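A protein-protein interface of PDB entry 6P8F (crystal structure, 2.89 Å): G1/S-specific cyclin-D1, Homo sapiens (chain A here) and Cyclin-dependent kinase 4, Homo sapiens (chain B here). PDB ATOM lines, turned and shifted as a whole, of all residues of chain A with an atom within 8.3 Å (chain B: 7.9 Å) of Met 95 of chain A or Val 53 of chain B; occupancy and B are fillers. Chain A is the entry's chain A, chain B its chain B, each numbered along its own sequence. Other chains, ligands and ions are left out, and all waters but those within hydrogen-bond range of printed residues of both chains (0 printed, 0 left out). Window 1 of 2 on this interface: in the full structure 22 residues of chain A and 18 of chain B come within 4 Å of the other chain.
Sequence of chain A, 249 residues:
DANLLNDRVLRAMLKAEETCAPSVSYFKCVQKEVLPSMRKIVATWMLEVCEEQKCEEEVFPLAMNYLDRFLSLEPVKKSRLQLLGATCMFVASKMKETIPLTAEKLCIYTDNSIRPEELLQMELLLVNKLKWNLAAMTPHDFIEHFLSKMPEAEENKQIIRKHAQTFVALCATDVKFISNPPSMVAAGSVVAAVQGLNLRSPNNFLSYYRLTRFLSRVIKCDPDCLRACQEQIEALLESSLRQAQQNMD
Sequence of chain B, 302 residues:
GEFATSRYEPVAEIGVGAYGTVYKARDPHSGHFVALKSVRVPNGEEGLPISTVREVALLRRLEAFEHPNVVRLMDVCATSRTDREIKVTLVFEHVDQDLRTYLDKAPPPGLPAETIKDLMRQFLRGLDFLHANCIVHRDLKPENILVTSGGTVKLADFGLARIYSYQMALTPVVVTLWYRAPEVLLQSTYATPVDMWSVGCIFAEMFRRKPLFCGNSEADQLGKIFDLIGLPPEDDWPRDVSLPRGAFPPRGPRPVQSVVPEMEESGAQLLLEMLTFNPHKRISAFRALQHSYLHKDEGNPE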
ATOM      1  N   GLU A  56      15.115 -23.274  32.728  1.00  0.00           N
ATOM      2  CA  GLU A  56      14.161 -22.188  32.613  1.00  0.00           C
ATOM      3  C   GLU A  56      12.774 -22.748  32.302  1.00  0.00           C
ATOM      4  O   GLU A  56      12.619 -23.872  31.815  1.00  0.00           O
ATOM      5  CB  GLU A  56      14.620 -21.201  31.540  1.00  0.00           C
ATOM      6  CG  GLU A  56      14.112 -19.780  31.707  1.00  0.00           C
ATOM      7  CD  GLU A  56      13.013 -19.448  30.709  1.00  0.00           C
ATOM      8  OE1 GLU A  56      12.799 -20.248  29.774  1.00  0.00           O
ATOM      9  OE2 GLU A  56      12.373 -18.384  30.849  1.00  0.00           O
ATOM     10  N   GLU A  58      10.358 -22.410  30.148  1.00  0.00           N
ATOM     11  CA  GLU A  58       9.854 -22.782  28.835  1.00  0.00           C
ATOM     12  C   GLU A  58      10.642 -23.891  28.161  1.00  0.00           C
ATOM     13  O   GLU A  58      10.222 -24.350  27.096  1.00  0.00           O
ATOM     14  CB  GLU A  58       9.836 -21.568  27.900  1.00  0.00           C
ATOM     15  CG  GLU A  58       9.345 -20.287  28.534  1.00  0.00           C
ATOM     16  CD  GLU A  58       9.961 -19.059  27.914  1.00  0.00           C
ATOM     17  OE1 GLU A  58       9.320 -18.466  27.025  1.00  0.00           O
ATOM     18  OE2 GLU A  58      11.072 -18.675  28.324  1.00  0.00           O
ATOM     19  N   VAL A  59      11.770 -24.317  28.731  1.00  0.00           N
ATOM     20  CA  VAL A  59      12.589 -25.331  28.071  1.00  0.00           C
ATOM     21  C   VAL A  59      11.764 -26.583  27.801  1.00  0.00           C
ATOM     22  O   VAL A  59      11.730 -27.097  26.676  1.00  0.00           O
ATOM     23  CB  VAL A  59      13.836 -25.646  28.915  1.00  0.00           C
ATOM     24  CG1 VAL A  59      14.619 -26.798  28.291  1.00  0.00           C
ATOM     25  CG2 VAL A  59      14.703 -24.412  29.051  1.00  0.00           C
ATOM     26  N   LEU A  62       8.716 -26.113  25.318  1.00  0.00           N
ATOM     27  CA  LEU A  62       9.278 -25.896  23.991  1.00  0.00           C
ATOM     28  C   LEU A  62       9.848 -27.189  23.424  1.00  0.00           C
ATOM     29  O   LEU A  62       9.637 -27.504  22.245  1.00  0.00           O
ATOM     30  CB  LEU A  62      10.352 -24.813  24.047  1.00  0.00           C
ATOM     31  CG  LEU A  62      10.996 -24.369  22.735  1.00  0.00           C
ATOM     32  CD1 LEU A  62       9.927 -24.032  21.705  1.00  0.00           C
ATOM     33  CD2 LEU A  62      11.914 -23.181  22.967  1.00  0.00           C
ATOM     34  N   TYR A  66       8.912 -29.154  19.898  1.00  0.00           N
ATOM     35  CA  TYR A  66       9.802 -29.708  18.881  1.00  0.00           C
ATOM     36  C   TYR A  66       9.526 -31.187  18.653  1.00  0.00           C
ATOM     37  O   TYR A  66       9.499 -31.650  17.507  1.00  0.00           O
ATOM     38  CB  TYR A  66      11.266 -29.505  19.281  1.00  0.00           C
ATOM     39  CG  TYR A  66      11.711 -28.060  19.431  1.00  0.00           C
ATOM     40  CD1 TYR A  66      11.024 -27.026  18.808  1.00  0.00           C
ATOM     41  CD2 TYR A  66      12.829 -27.733  20.194  1.00  0.00           C
ATOM     42  CE1 TYR A  66      11.435 -25.712  18.944  1.00  0.00           C
ATOM     43  CE2 TYR A  66      13.244 -26.420  20.333  1.00  0.00           C
ATOM     44  CZ  TYR A  66      12.544 -25.416  19.706  1.00  0.00           C
ATOM     45  OH  TYR A  66      12.950 -24.111  19.843  1.00  0.00           O
ATOM     46  N   CYS A  88      15.646 -32.566  21.726  1.00  0.00           N
ATOM     47  CA  CYS A  88      14.739 -31.431  21.817  1.00  0.00           C
ATOM     48  C   CYS A  88      15.058 -30.572  23.033  1.00  0.00           C
ATOM     49  O   CYS A  88      15.078 -29.339  22.944  1.00  0.00           O
ATOM     50  CB  CYS A  88      13.297 -31.929  21.855  1.00  0.00           C
ATOM     51  SG  CYS A  88      12.765 -32.690  20.306  1.00  0.00           S
ATOM     52  N   MET A  89      15.321 -31.202  24.178  1.00  0.00           N
ATOM     53  CA  MET A  89      15.769 -30.444  25.339  1.00  0.00           C
ATOM     54  C   MET A  89      17.057 -29.692  25.027  1.00  0.00           C
ATOM     55  O   MET A  89      17.208 -28.522  25.396  1.00  0.00           O
ATOM     56  CB  MET A  89      15.959 -31.380  26.532  1.00  0.00           C
ATOM     57  CG  MET A  89      14.671 -32.009  27.033  1.00  0.00           C
ATOM     58  SD  MET A  89      14.876 -32.885  28.597  1.00  0.00           S
ATOM     59  CE  MET A  89      15.774 -34.346  28.082  1.00  0.00           C
ATOM     60  N   PHE A  90      17.984 -30.349  24.328  1.00  0.00           N
ATOM     61  CA  PHE A  90      19.250 -29.732  23.941  1.00  0.00           C
ATOM     62  C   PHE A  90      19.021 -28.409  23.220  1.00  0.00           C
ATOM     63  O   PHE A  90      19.538 -27.361  23.626  1.00  0.00           O
ATOM     64  CB  PHE A  90      20.028 -30.711  23.058  1.00  0.00           C
ATOM     65  CG  PHE A  90      21.465 -30.343  22.838  1.00  0.00           C
ATOM     66  CD1 PHE A  90      22.293 -30.041  23.905  1.00  0.00           C
ATOM     67  CD2 PHE A  90      22.000 -30.339  21.554  1.00  0.00           C
ATOM     68  CE1 PHE A  90      23.627 -29.724  23.695  1.00  0.00           C
ATOM     69  CE2 PHE A  90      23.329 -30.022  21.338  1.00  0.00           C
ATOM     70  CZ  PHE A  90      24.145 -29.715  22.408  1.00  0.00           C
ATOM     71  N   VAL A  91      18.228 -28.441  22.147  1.00  0.00           N
ATOM     72  CA  VAL A  91      17.998 -27.237  21.355  1.00  0.00           C
ATOM     73  C   VAL A  91      17.186 -26.221  22.146  1.00  0.00           C
ATOM     74  O   VAL A  91      17.520 -25.031  22.179  1.00  0.00           O
ATOM     75  CB  VAL A  91      17.314 -27.591  20.023  1.00  0.00           C
ATOM     76  CG1 VAL A  91      16.730 -26.345  19.389  1.00  0.00           C
ATOM     77  CG2 VAL A  91      18.300 -28.262  19.083  1.00  0.00           C
ATOM     78  N   ALA A  92      16.112 -26.671  22.797  1.00  0.00           N
ATOM     79  CA  ALA A  92      15.286 -25.749  23.570  1.00  0.00           C
ATOM     80  C   ALA A  92      16.108 -25.047  24.640  1.00  0.00           C
ATOM     81  O   ALA A  92      15.922 -23.849  24.891  1.00  0.00           O
ATOM     82  CB  ALA A  92      14.104 -26.495  24.193  1.00  0.00           C
ATOM     83  N   SER A  93      17.034 -25.772  25.270  1.00  0.00           N
ATOM     84  CA  SER A  93      17.916 -25.150  26.250  1.00  0.00           C
ATOM     85  C   SER A  93      18.720 -24.024  25.615  1.00  0.00           C
ATOM     86  O   SER A  93      18.900 -22.960  26.218  1.00  0.00           O
ATOM     87  CB  SER A  93      18.843 -26.202  26.857  1.00  0.00           C
ATOM     88  OG  SER A  93      19.284 -25.814  28.146  1.00  0.00           O
ATOM     89  N   LYS A  94      19.198 -24.233  24.386  1.00  0.00           N
ATOM     90  CA  LYS A  94      19.960 -23.190  23.712  1.00  0.00           C
ATOM     91  C   LYS A  94      19.101 -21.968  23.427  1.00  0.00           C
ATOM     92  O   LYS A  94      19.589 -20.833  23.492  1.00  0.00           O
ATOM     93  CB  LYS A  94      20.559 -23.730  22.414  1.00  0.00           C
ATOM     94  CG  LYS A  94      21.473 -24.931  22.605  1.00  0.00           C
ATOM     95  CD  LYS A  94      22.203 -25.275  21.310  1.00  0.00           C
ATOM     96  CE  LYS A  94      23.157 -26.441  21.514  1.00  0.00           C
ATOM     97  NZ  LYS A  94      24.041 -26.664  20.334  1.00  0.00           N
ATOM     98  N   MET A  95      17.819 -22.175  23.131  1.00  0.00           N
ATOM     99  CA  MET A  95      16.946 -21.085  22.722  1.00  0.00           C
ATOM    100  C   MET A  95      16.479 -20.215  23.882  1.00  0.00           C
ATOM    101  O   MET A  95      16.048 -19.082  23.646  1.00  0.00           O
ATOM    102  CB  MET A  95      15.726 -21.648  21.993  1.00  0.00           C
ATOM    103  CG  MET A  95      16.038 -22.232  20.628  1.00  0.00           C
ATOM    104  SD  MET A  95      16.227 -20.957  19.366  1.00  0.00           S
ATOM    105  CE  MET A  95      14.794 -19.942  19.711  1.00  0.00           C
ATOM    106  N   LYS A  96      16.536 -20.714  25.120  1.00  0.00           N
ATOM    107  CA  LYS A  96      15.946 -19.986  26.238  1.00  0.00           C
ATOM    108  C   LYS A  96      16.810 -19.931  27.491  1.00  0.00           C
ATOM    109  O   LYS A  96      16.429 -19.238  28.440  1.00  0.00           O
ATOM    110  CB  LYS A  96      14.580 -20.592  26.607  1.00  0.00           C
ATOM    111  CG  LYS A  96      13.636 -20.790  25.426  1.00  0.00           C
ATOM    112  CD  LYS A  96      12.454 -19.828  25.432  1.00  0.00           C
ATOM    113  CE  LYS A  96      12.671 -18.672  24.479  1.00  0.00           C
ATOM    114  NZ  LYS A  96      11.428 -17.875  24.322  1.00  0.00           N
ATOM    115  N   GLU A  97      17.948 -20.612  27.541  1.00  0.00           N
ATOM    116  CA  GLU A  97      18.783 -20.642  28.732  1.00  0.00           C
ATOM    117  C   GLU A  97      20.113 -19.956  28.463  1.00  0.00           C
ATOM    118  O   GLU A  97      20.665 -20.060  27.362  1.00  0.00           O
ATOM    119  CB  GLU A  97      19.029 -22.077  29.196  1.00  0.00           C
ATOM    120  CG  GLU A  97      17.777 -22.793  29.642  1.00  0.00           C
ATOM    121  CD  GLU A  97      18.035 -23.747  30.782  1.00  0.00           C
ATOM    122  OE1 GLU A  97      18.368 -24.922  30.516  1.00  0.00           O
ATOM    123  OE2 GLU A  97      17.922 -23.316  31.948  1.00  0.00           O
ATOM    124  N   THR A  98      20.626 -19.260  29.479  1.00  0.00           N
ATOM    125  CA  THR A  98      21.906 -18.576  29.333  1.00  0.00           C
ATOM    126  C   THR A  98      23.032 -19.577  29.107  1.00  0.00           C
ATOM    127  O   THR A  98      23.796 -19.461  28.141  1.00  0.00           O
ATOM    128  CB  THR A  98      22.181 -17.711  30.563  1.00  0.00           C
ATOM    129  OG1 THR A  98      21.137 -16.737  30.706  1.00  0.00           O
ATOM    130  CG2 THR A  98      23.513 -16.997  30.422  1.00  0.00           C
ATOM    131  N   PRO A 100      23.219 -23.419  28.392  1.00  0.00           N
ATOM    132  CA  PRO A 100      22.324 -24.543  28.101  1.00  0.00           C
ATOM    133  C   PRO A 100      22.830 -25.848  28.693  1.00  0.00           C
ATOM    134  O   PRO A 100      23.965 -25.972  29.159  1.00  0.00           O
ATOM    135  CB  PRO A 100      22.309 -24.603  26.571  1.00  0.00           C
ATOM    136  CG  PRO A 100      22.787 -23.275  26.126  1.00  0.00           C
ATOM    137  CD  PRO A 100      23.771 -22.833  27.167  1.00  0.00           C
ATOM    138  N   GLU A 123      20.754 -33.396  16.452  1.00  0.00           N
ATOM    139  CA  GLU A 123      20.444 -31.970  16.479  1.00  0.00           C
ATOM    140  C   GLU A 123      20.286 -31.413  15.069  1.00  0.00           C
ATOM    141  O   GLU A 123      19.373 -30.620  14.808  1.00  0.00           O
ATOM    142  CB  GLU A 123      21.530 -31.208  17.243  1.00  0.00           C
ATOM    143  CG  GLU A 123      21.208 -29.741  17.477  1.00  0.00           C
ATOM    144  CD  GLU A 123      22.408 -28.937  17.954  1.00  0.00           C
ATOM    145  OE1 GLU A 123      23.518 -29.124  17.408  1.00  0.00           O
ATOM    146  OE2 GLU A 123      22.234 -28.108  18.873  1.00  0.00           O
ATOM    147  N   VAL A 127      16.837 -29.871  13.622  1.00  0.00           N
ATOM    148  CA  VAL A 127      16.742 -28.470  13.232  1.00  0.00           C
ATOM    149  C   VAL A 127      16.367 -28.345  11.764  1.00  0.00           C
ATOM    150  O   VAL A 127      15.543 -27.504  11.391  1.00  0.00           O
ATOM    151  CB  VAL A 127      18.061 -27.747  13.546  1.00  0.00           C
ATOM    152  CG1 VAL A 127      18.083 -26.407  12.874  1.00  0.00           C
ATOM    153  CG2 VAL A 127      18.217 -27.578  15.042  1.00  0.00           C
ATOM    154  N   TRP A 132      14.575 -24.851  10.634  1.00  0.00           N
ATOM    155  CA  TRP A 132      15.100 -23.852  11.562  1.00  0.00           C
ATOM    156  C   TRP A 132      14.009 -22.962  12.154  1.00  0.00           C
ATOM    157  O   TRP A 132      14.291 -21.851  12.617  1.00  0.00           O
ATOM    158  CB  TRP A 132      16.183 -22.993  10.900  1.00  0.00           C
ATOM    159  CG  TRP A 132      17.444 -23.752  10.610  1.00  0.00           C
ATOM    160  CD1 TRP A 132      17.613 -24.729   9.674  1.00  0.00           C
ATOM    161  CD2 TRP A 132      18.713 -23.594  11.258  1.00  0.00           C
ATOM    162  NE1 TRP A 132      18.907 -25.190   9.698  1.00  0.00           N
ATOM    163  CE2 TRP A 132      19.603 -24.510  10.661  1.00  0.00           C
ATOM    164  CE3 TRP A 132      19.182 -22.774  12.289  1.00  0.00           C
ATOM    165  CZ2 TRP A 132      20.934 -24.627  11.061  1.00  0.00           C
ATOM    166  CZ3 TRP A 132      20.505 -22.887  12.681  1.00  0.00           C
ATOM    167  CH2 TRP A 132      21.365 -23.809  12.070  1.00  0.00           C
ATOM    168  N   ASN A 133      12.762 -23.431  12.169  1.00  0.00           N
ATOM    169  CA  ASN A 133      11.660 -22.693  12.783  1.00  0.00           C
ATOM    170  C   ASN A 133      11.602 -23.054  14.265  1.00  0.00           C
ATOM    171  O   ASN A 133      10.797 -23.872  14.712  1.00  0.00           O
ATOM    172  CB  ASN A 133      10.350 -23.010  12.077  1.00  0.00           C
ATOM    173  CG  ASN A 133      10.011 -22.002  11.015  1.00  0.00           C
ATOM    174  OD1 ASN A 133      10.117 -22.280   9.820  1.00  0.00           O
ATOM    175  ND2 ASN A 133       9.599 -20.815  11.443  1.00  0.00           N
ATOM    176  N   LEU A 134      12.471 -22.412  15.046  1.00  0.00           N
ATOM    177  CA  LEU A 134      12.635 -22.760  16.449  1.00  0.00           C
ATOM    178  C   LEU A 134      12.128 -21.703  17.419  1.00  0.00           C
ATOM    179  O   LEU A 134      12.018 -21.995  18.616  1.00  0.00           O
ATOM    180  CB  LEU A 134      14.114 -23.049  16.748  1.00  0.00           C
ATOM    181  CG  LEU A 134      14.726 -24.054  15.773  1.00  0.00           C
ATOM    182  CD1 LEU A 134      16.154 -24.365  16.147  1.00  0.00           C
ATOM    183  CD2 LEU A 134      13.895 -25.328  15.733  1.00  0.00           C
ATOM    184  N   ALA A 135      11.813 -20.496  16.952  1.00  0.00           N
ATOM    185  CA  ALA A 135      11.297 -19.445  17.831  1.00  0.00           C
ATOM    186  C   ALA A 135       9.771 -19.540  17.905  1.00  0.00           C
ATOM    187  O   ALA A 135       9.027 -18.657  17.470  1.00  0.00           O
ATOM    188  CB  ALA A 135      11.754 -18.074  17.348  1.00  0.00           C
ATOM    189  N   ALA A 136       9.311 -20.644  18.487  1.00  0.00           N
ATOM    190  CA  ALA A 136       7.882 -20.913  18.579  1.00  0.00           C
ATOM    191  C   ALA A 136       7.261 -20.112  19.712  1.00  0.00           C
ATOM    192  O   ALA A 136       7.881 -19.905  20.760  1.00  0.00           O
ATOM    193  CB  ALA A 136       7.624 -22.404  18.797  1.00  0.00           C
ATOM    194  N   VAL B  41      30.444 -22.046  10.714  1.00  0.00           N
ATOM    195  CA  VAL B  41      30.439 -21.915  12.169  1.00  0.00           C
ATOM    196  C   VAL B  41      31.370 -22.970  12.758  1.00  0.00           C
ATOM    197  O   VAL B  41      31.550 -24.040  12.156  1.00  0.00           O
ATOM    198  CB  VAL B  41      29.013 -22.033  12.732  1.00  0.00           C
ATOM    199  CG1 VAL B  41      28.128 -20.932  12.156  1.00  0.00           C
ATOM    200  CG2 VAL B  41      28.431 -23.402  12.432  1.00  0.00           C
ATOM    201  N   LEU B  48      25.679 -27.098  17.497  1.00  0.00           N
ATOM    202  CA  LEU B  48      25.481 -25.791  16.890  1.00  0.00           C
ATOM    203  C   LEU B  48      25.598 -24.697  17.948  1.00  0.00           C
ATOM    204  O   LEU B  48      25.120 -24.870  19.074  1.00  0.00           O
ATOM    205  CB  LEU B  48      24.116 -25.717  16.207  1.00  0.00           C
ATOM    206  CG  LEU B  48      23.968 -26.495  14.898  1.00  0.00           C
ATOM    207  CD1 LEU B  48      22.507 -26.796  14.632  1.00  0.00           C
ATOM    208  CD2 LEU B  48      24.576 -25.733  13.728  1.00  0.00           C
ATOM    209  N   PRO B  49      26.221 -23.568  17.625  1.00  0.00           N
ATOM    210  CA  PRO B  49      26.368 -22.495  18.613  1.00  0.00           C
ATOM    211  C   PRO B  49      25.030 -21.856  18.959  1.00  0.00           C
ATOM    212  O   PRO B  49      24.073 -21.880  18.183  1.00  0.00           O
ATOM    213  CB  PRO B  49      27.298 -21.492  17.919  1.00  0.00           C
ATOM    214  CG  PRO B  49      27.919 -22.255  16.774  1.00  0.00           C
ATOM    215  CD  PRO B  49      26.881 -23.238  16.352  1.00  0.00           C
ATOM    216  N   ILE B  50      24.980 -21.278  20.162  1.00  0.00           N
ATOM    217  CA  ILE B  50      23.746 -20.660  20.640  1.00  0.00           C
ATOM    218  C   ILE B  50      23.332 -19.521  19.719  1.00  0.00           C
ATOM    219  O   ILE B  50      22.169 -19.421  19.311  1.00  0.00           O
ATOM    220  CB  ILE B  50      23.910 -20.168  22.088  1.00  0.00           C
ATOM    221  CG1 ILE B  50      24.464 -21.276  22.976  1.00  0.00           C
ATOM    222  CG2 ILE B  50      22.579 -19.665  22.637  1.00  0.00           C
ATOM    223  CD1 ILE B  50      24.684 -20.829  24.392  1.00  0.00           C
ATOM    224  N   SER B  51      24.276 -18.641  19.382  1.00  0.00           N
ATOM    225  CA  SER B  51      23.938 -17.489  18.555  1.00  0.00           C
ATOM    226  C   SER B  51      23.450 -17.924  17.181  1.00  0.00           C
ATOM    227  O   SER B  51      22.477 -17.369  16.658  1.00  0.00           O
ATOM    228  CB  SER B  51      25.144 -16.558  18.426  1.00  0.00           C
ATOM    229  OG  SER B  51      26.251 -17.236  17.859  1.00  0.00           O
ATOM    230  N   THR B  52      24.104 -18.921  16.584  1.00  0.00           N
ATOM    231  CA  THR B  52      23.690 -19.374  15.262  1.00  0.00           C
ATOM    232  C   THR B  52      22.255 -19.869  15.283  1.00  0.00           C
ATOM    233  O   THR B  52      21.450 -19.508  14.416  1.00  0.00           O
ATOM    234  CB  THR B  52      24.619 -20.476  14.762  1.00  0.00           C
ATOM    235  OG1 THR B  52      25.926 -19.936  14.545  1.00  0.00           O
ATOM    236  CG2 THR B  52      24.088 -21.060  13.459  1.00  0.00           C
ATOM    237  N   VAL B  53      21.911 -20.678  16.282  1.00  0.00           N
ATOM    238  CA  VAL B  53      20.577 -21.256  16.330  1.00  0.00           C
ATOM    239  C   VAL B  53      19.541 -20.213  16.745  1.00  0.00           C
ATOM    240  O   VAL B  53      18.361 -20.337  16.400  1.00  0.00           O
ATOM    241  CB  VAL B  53      20.577 -22.480  17.264  1.00  0.00           C
ATOM    242  CG1 VAL B  53      20.541 -22.054  18.726  1.00  0.00           C
ATOM    243  CG2 VAL B  53      19.419 -23.381  16.941  1.00  0.00           C
ATOM    244  N   ARG B  54      19.952 -19.167  17.463  1.00  0.00           N
ATOM    245  CA  ARG B  54      19.008 -18.121  17.846  1.00  0.00           C
ATOM    246  C   ARG B  54      18.792 -17.132  16.708  1.00  0.00           C
ATOM    247  O   ARG B  54      17.650 -16.782  16.389  1.00  0.00           O
ATOM    248  CB  ARG B  54      19.502 -17.386  19.095  1.00  0.00           C
ATOM    249  CG  ARG B  54      19.019 -17.961  20.413  1.00  0.00           C
ATOM    250  CD  ARG B  54      19.743 -17.322  21.591  1.00  0.00           C
ATOM    251  NE  ARG B  54      19.231 -17.794  22.877  1.00  0.00           N
ATOM    252  CZ  ARG B  54      19.840 -17.606  24.042  1.00  0.00           C
ATOM    253  NH1 ARG B  54      20.989 -16.952  24.089  1.00  0.00           N
ATOM    254  NH2 ARG B  54      19.304 -18.070  25.161  1.00  0.00           N
ATOM    255  N   GLU B  55      19.878 -16.669  16.084  1.00  0.00           N
ATOM    256  CA  GLU B  55      19.754 -15.653  15.044  1.00  0.00           C
ATOM    257  C   GLU B  55      18.991 -16.181  13.833  1.00  0.00           C
ATOM    258  O   GLU B  55      18.126 -15.486  13.289  1.00  0.00           O
ATOM    259  CB  GLU B  55      21.137 -15.146  14.632  1.00  0.00           C
ATOM    260  CG  GLU B  55      21.859 -14.370  15.728  1.00  0.00           C
ATOM    261  CD  GLU B  55      23.300 -14.033  15.372  1.00  0.00           C
ATOM    262  OE1 GLU B  55      23.710 -14.256  14.212  1.00  0.00           O
ATOM    263  OE2 GLU B  55      24.026 -13.541  16.261  1.00  0.00           O
ATOM    264  N   VAL B  56      19.291 -17.406  13.398  1.00  0.00           N
ATOM    265  CA  VAL B  56      18.607 -17.952  12.228  1.00  0.00           C
ATOM    266  C   VAL B  56      17.134 -18.188  12.532  1.00  0.00           C
ATOM    267  O   VAL B  56      16.264 -17.944  11.686  1.00  0.00           O
ATOM    268  CB  VAL B  56      19.300 -19.242  11.751  1.00  0.00           C
ATOM    269  CG1 VAL B  56      18.545 -19.844  10.580  1.00  0.00           C
ATOM    270  CG2 VAL B  56      20.737 -18.954  11.359  1.00  0.00           C
ATOM    271  N   ALA B  57      16.827 -18.665  13.740  1.00  0.00           N
ATOM    272  CA  ALA B  57      15.433 -18.882  14.112  1.00  0.00           C
ATOM    273  C   ALA B  57      14.658 -17.571  14.129  1.00  0.00           C
ATOM    274  O   ALA B  57      13.486 -17.530  13.733  1.00  0.00           O
ATOM    275  CB  ALA B  57      15.355 -19.571  15.472  1.00  0.00           C
ATOM    276  N   LEU B  58      15.297 -16.487  14.580  1.00  0.00           N
ATOM    277  CA  LEU B  58      14.640 -15.185  14.587  1.00  0.00           C
ATOM    278  C   LEU B  58      14.300 -14.737  13.174  1.00  0.00           C
ATOM    279  O   LEU B  58      13.225 -14.176  12.935  1.00  0.00           O
ATOM    280  CB  LEU B  58      15.526 -14.154  15.278  1.00  0.00           C
ATOM    281  CG  LEU B  58      15.114 -12.691  15.095  1.00  0.00           C
ATOM    282  CD1 LEU B  58      14.005 -12.304  16.069  1.00  0.00           C
ATOM    283  CD2 LEU B  58      16.323 -11.777  15.245  1.00  0.00           C
ATOM    284  N   LEU B  59      15.206 -14.978  12.223  1.00  0.00           N
ATOM    285  CA  LEU B  59      14.884 -14.704  10.827  1.00  0.00           C
ATOM    286  C   LEU B  59      13.714 -15.561  10.360  1.00  0.00           C
ATOM    287  O   LEU B  59      12.836 -15.079   9.638  1.00  0.00           O
ATOM    288  CB  LEU B  59      16.111 -14.927   9.940  1.00  0.00           C
ATOM    289  CG  LEU B  59      17.222 -13.874  10.019  1.00  0.00           C
ATOM    290  CD1 LEU B  59      18.153 -14.006   8.823  1.00  0.00           C
ATOM    291  CD2 LEU B  59      16.661 -12.455  10.121  1.00  0.00           C
ATOM    292  N   VAL B  88      26.331 -23.189   7.251  1.00  0.00           N
ATOM    293  CA  VAL B  88      24.928 -22.797   7.201  1.00  0.00           C
ATOM    294  C   VAL B  88      24.756 -21.836   6.031  1.00  0.00           C
ATOM    295  O   VAL B  88      25.367 -20.759   6.005  1.00  0.00           O
ATOM    296  CB  VAL B  88      24.468 -22.154   8.519  1.00  0.00           C
ATOM    297  CG1 VAL B  88      22.964 -21.987   8.529  1.00  0.00           C
ATOM    298  CG2 VAL B  88      24.904 -22.991   9.705  1.00  0.00           C
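O of Glu 97 of chain A is in hydrogen-bond range of NH2 of Arg 54 of chain B (3.3 Å). NZ of Lys 94 of chain A is in hydrogen-bond range of O of Leu 48 of chain B. N of Leu 48 of chain B sits at hydrogen-bond distance from OE1 of Glu 123 of chain A (3.0 Å). O of Lys 94 of chain A is in hydrogen-bond range of NE of Arg 54 of chain B, 3.1 Å away. The side-chain sulfur (SD) of Met 95 of chain A lies close to the backbone carbonyl oxygen (O) of Val 53 of chain B (3.7 Å).
The side-chain hydroxyl (OG) of Ser 93 of chain A lies within hydrogen-bond range of the side-chain carboxylate (OE1) of Glu 97 of chain A (2.7 Å). N of Glu 56 of chain A lies within hydrogen-bond range of OE2 of Glu 97 of chain A, 2.9 Å away. The backbone NH of Trp 132 of chain A sits at hydrogen-bond distance from the backbone carbonyl oxygen of Val 127 of chain A, 2.9 Å away. NZ of Lys 96 of chain A lies within salt-bridge range of OE1 of Glu 58 of chain A (3.5 Å).
Val 91 of chain A touches none of the printed residues of chain B. Met 95 of chain A touches two residues of chain B. Of the printed residues of chain A, Ile 50 of chain B touches Lys 94 and Pro 100. Of the printed residues of chain A, Val 56 of chain B touches Trp 132 (3.5 Å). The nearest residue of chain B that does not touch Met 95 of chain A is Ala 57 of chain B (4.2 Å). The nearest printed residue of chain A that does not touch Val 53 of chain B is Lys 94 of chain A (4.1 Å). The nearest printed residue of chain B that does not touch Lys 94 of chain A is Val 53 of chain B (4.1 Å).
Lys 94 of chain A touches Ile 50 of chain B (O to CG2, 3.3 Å). Arg 54 of chain B touches Met 95 of chain A (NE to O, 3.5 Å). Arg 54 of chain B touches Lys 96 of chain A (NH2 to N, 3.8 Å). CD of Pro 100 of chain A touches CD1 of Ile 50 of chain B, at 3.5 Å. O of Thr 52 of chain B touches CZ3 of Trp 132 of chain A, 3.9 Å away. Val 53 of chain B touches Trp 132 of chain A (CA to CZ3, 3.998 Å). Trp 132 of chain A touches Val 56 of chain B. Ala 57 of chain B touches Trp 132 of chain A. Val 53 of chain B touches Leu 134 of chain A. Ala 135 of chain A touches Ala 57 of chain B (N to CB, 3.9 Å).
Hydrophobic or aromatic side chains of chain A within 4 Å of the printed part of chain B: Met 95, Pro 100, Trp 132 and Leu 134. Along chain A the printed residues that touch a printed residue of chain B span positions 94 to 135. Hydrophobic or aromatic side chains of chain B within 4 Å of the printed part of chain A: Leu 48, Ile 50, Val 53, Val 56 and Ala 57. Among the printed residues, no Asp or Glu carboxylate lies within 4 Å of a Lys or Arg side-chain nitrogen of the other chain.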
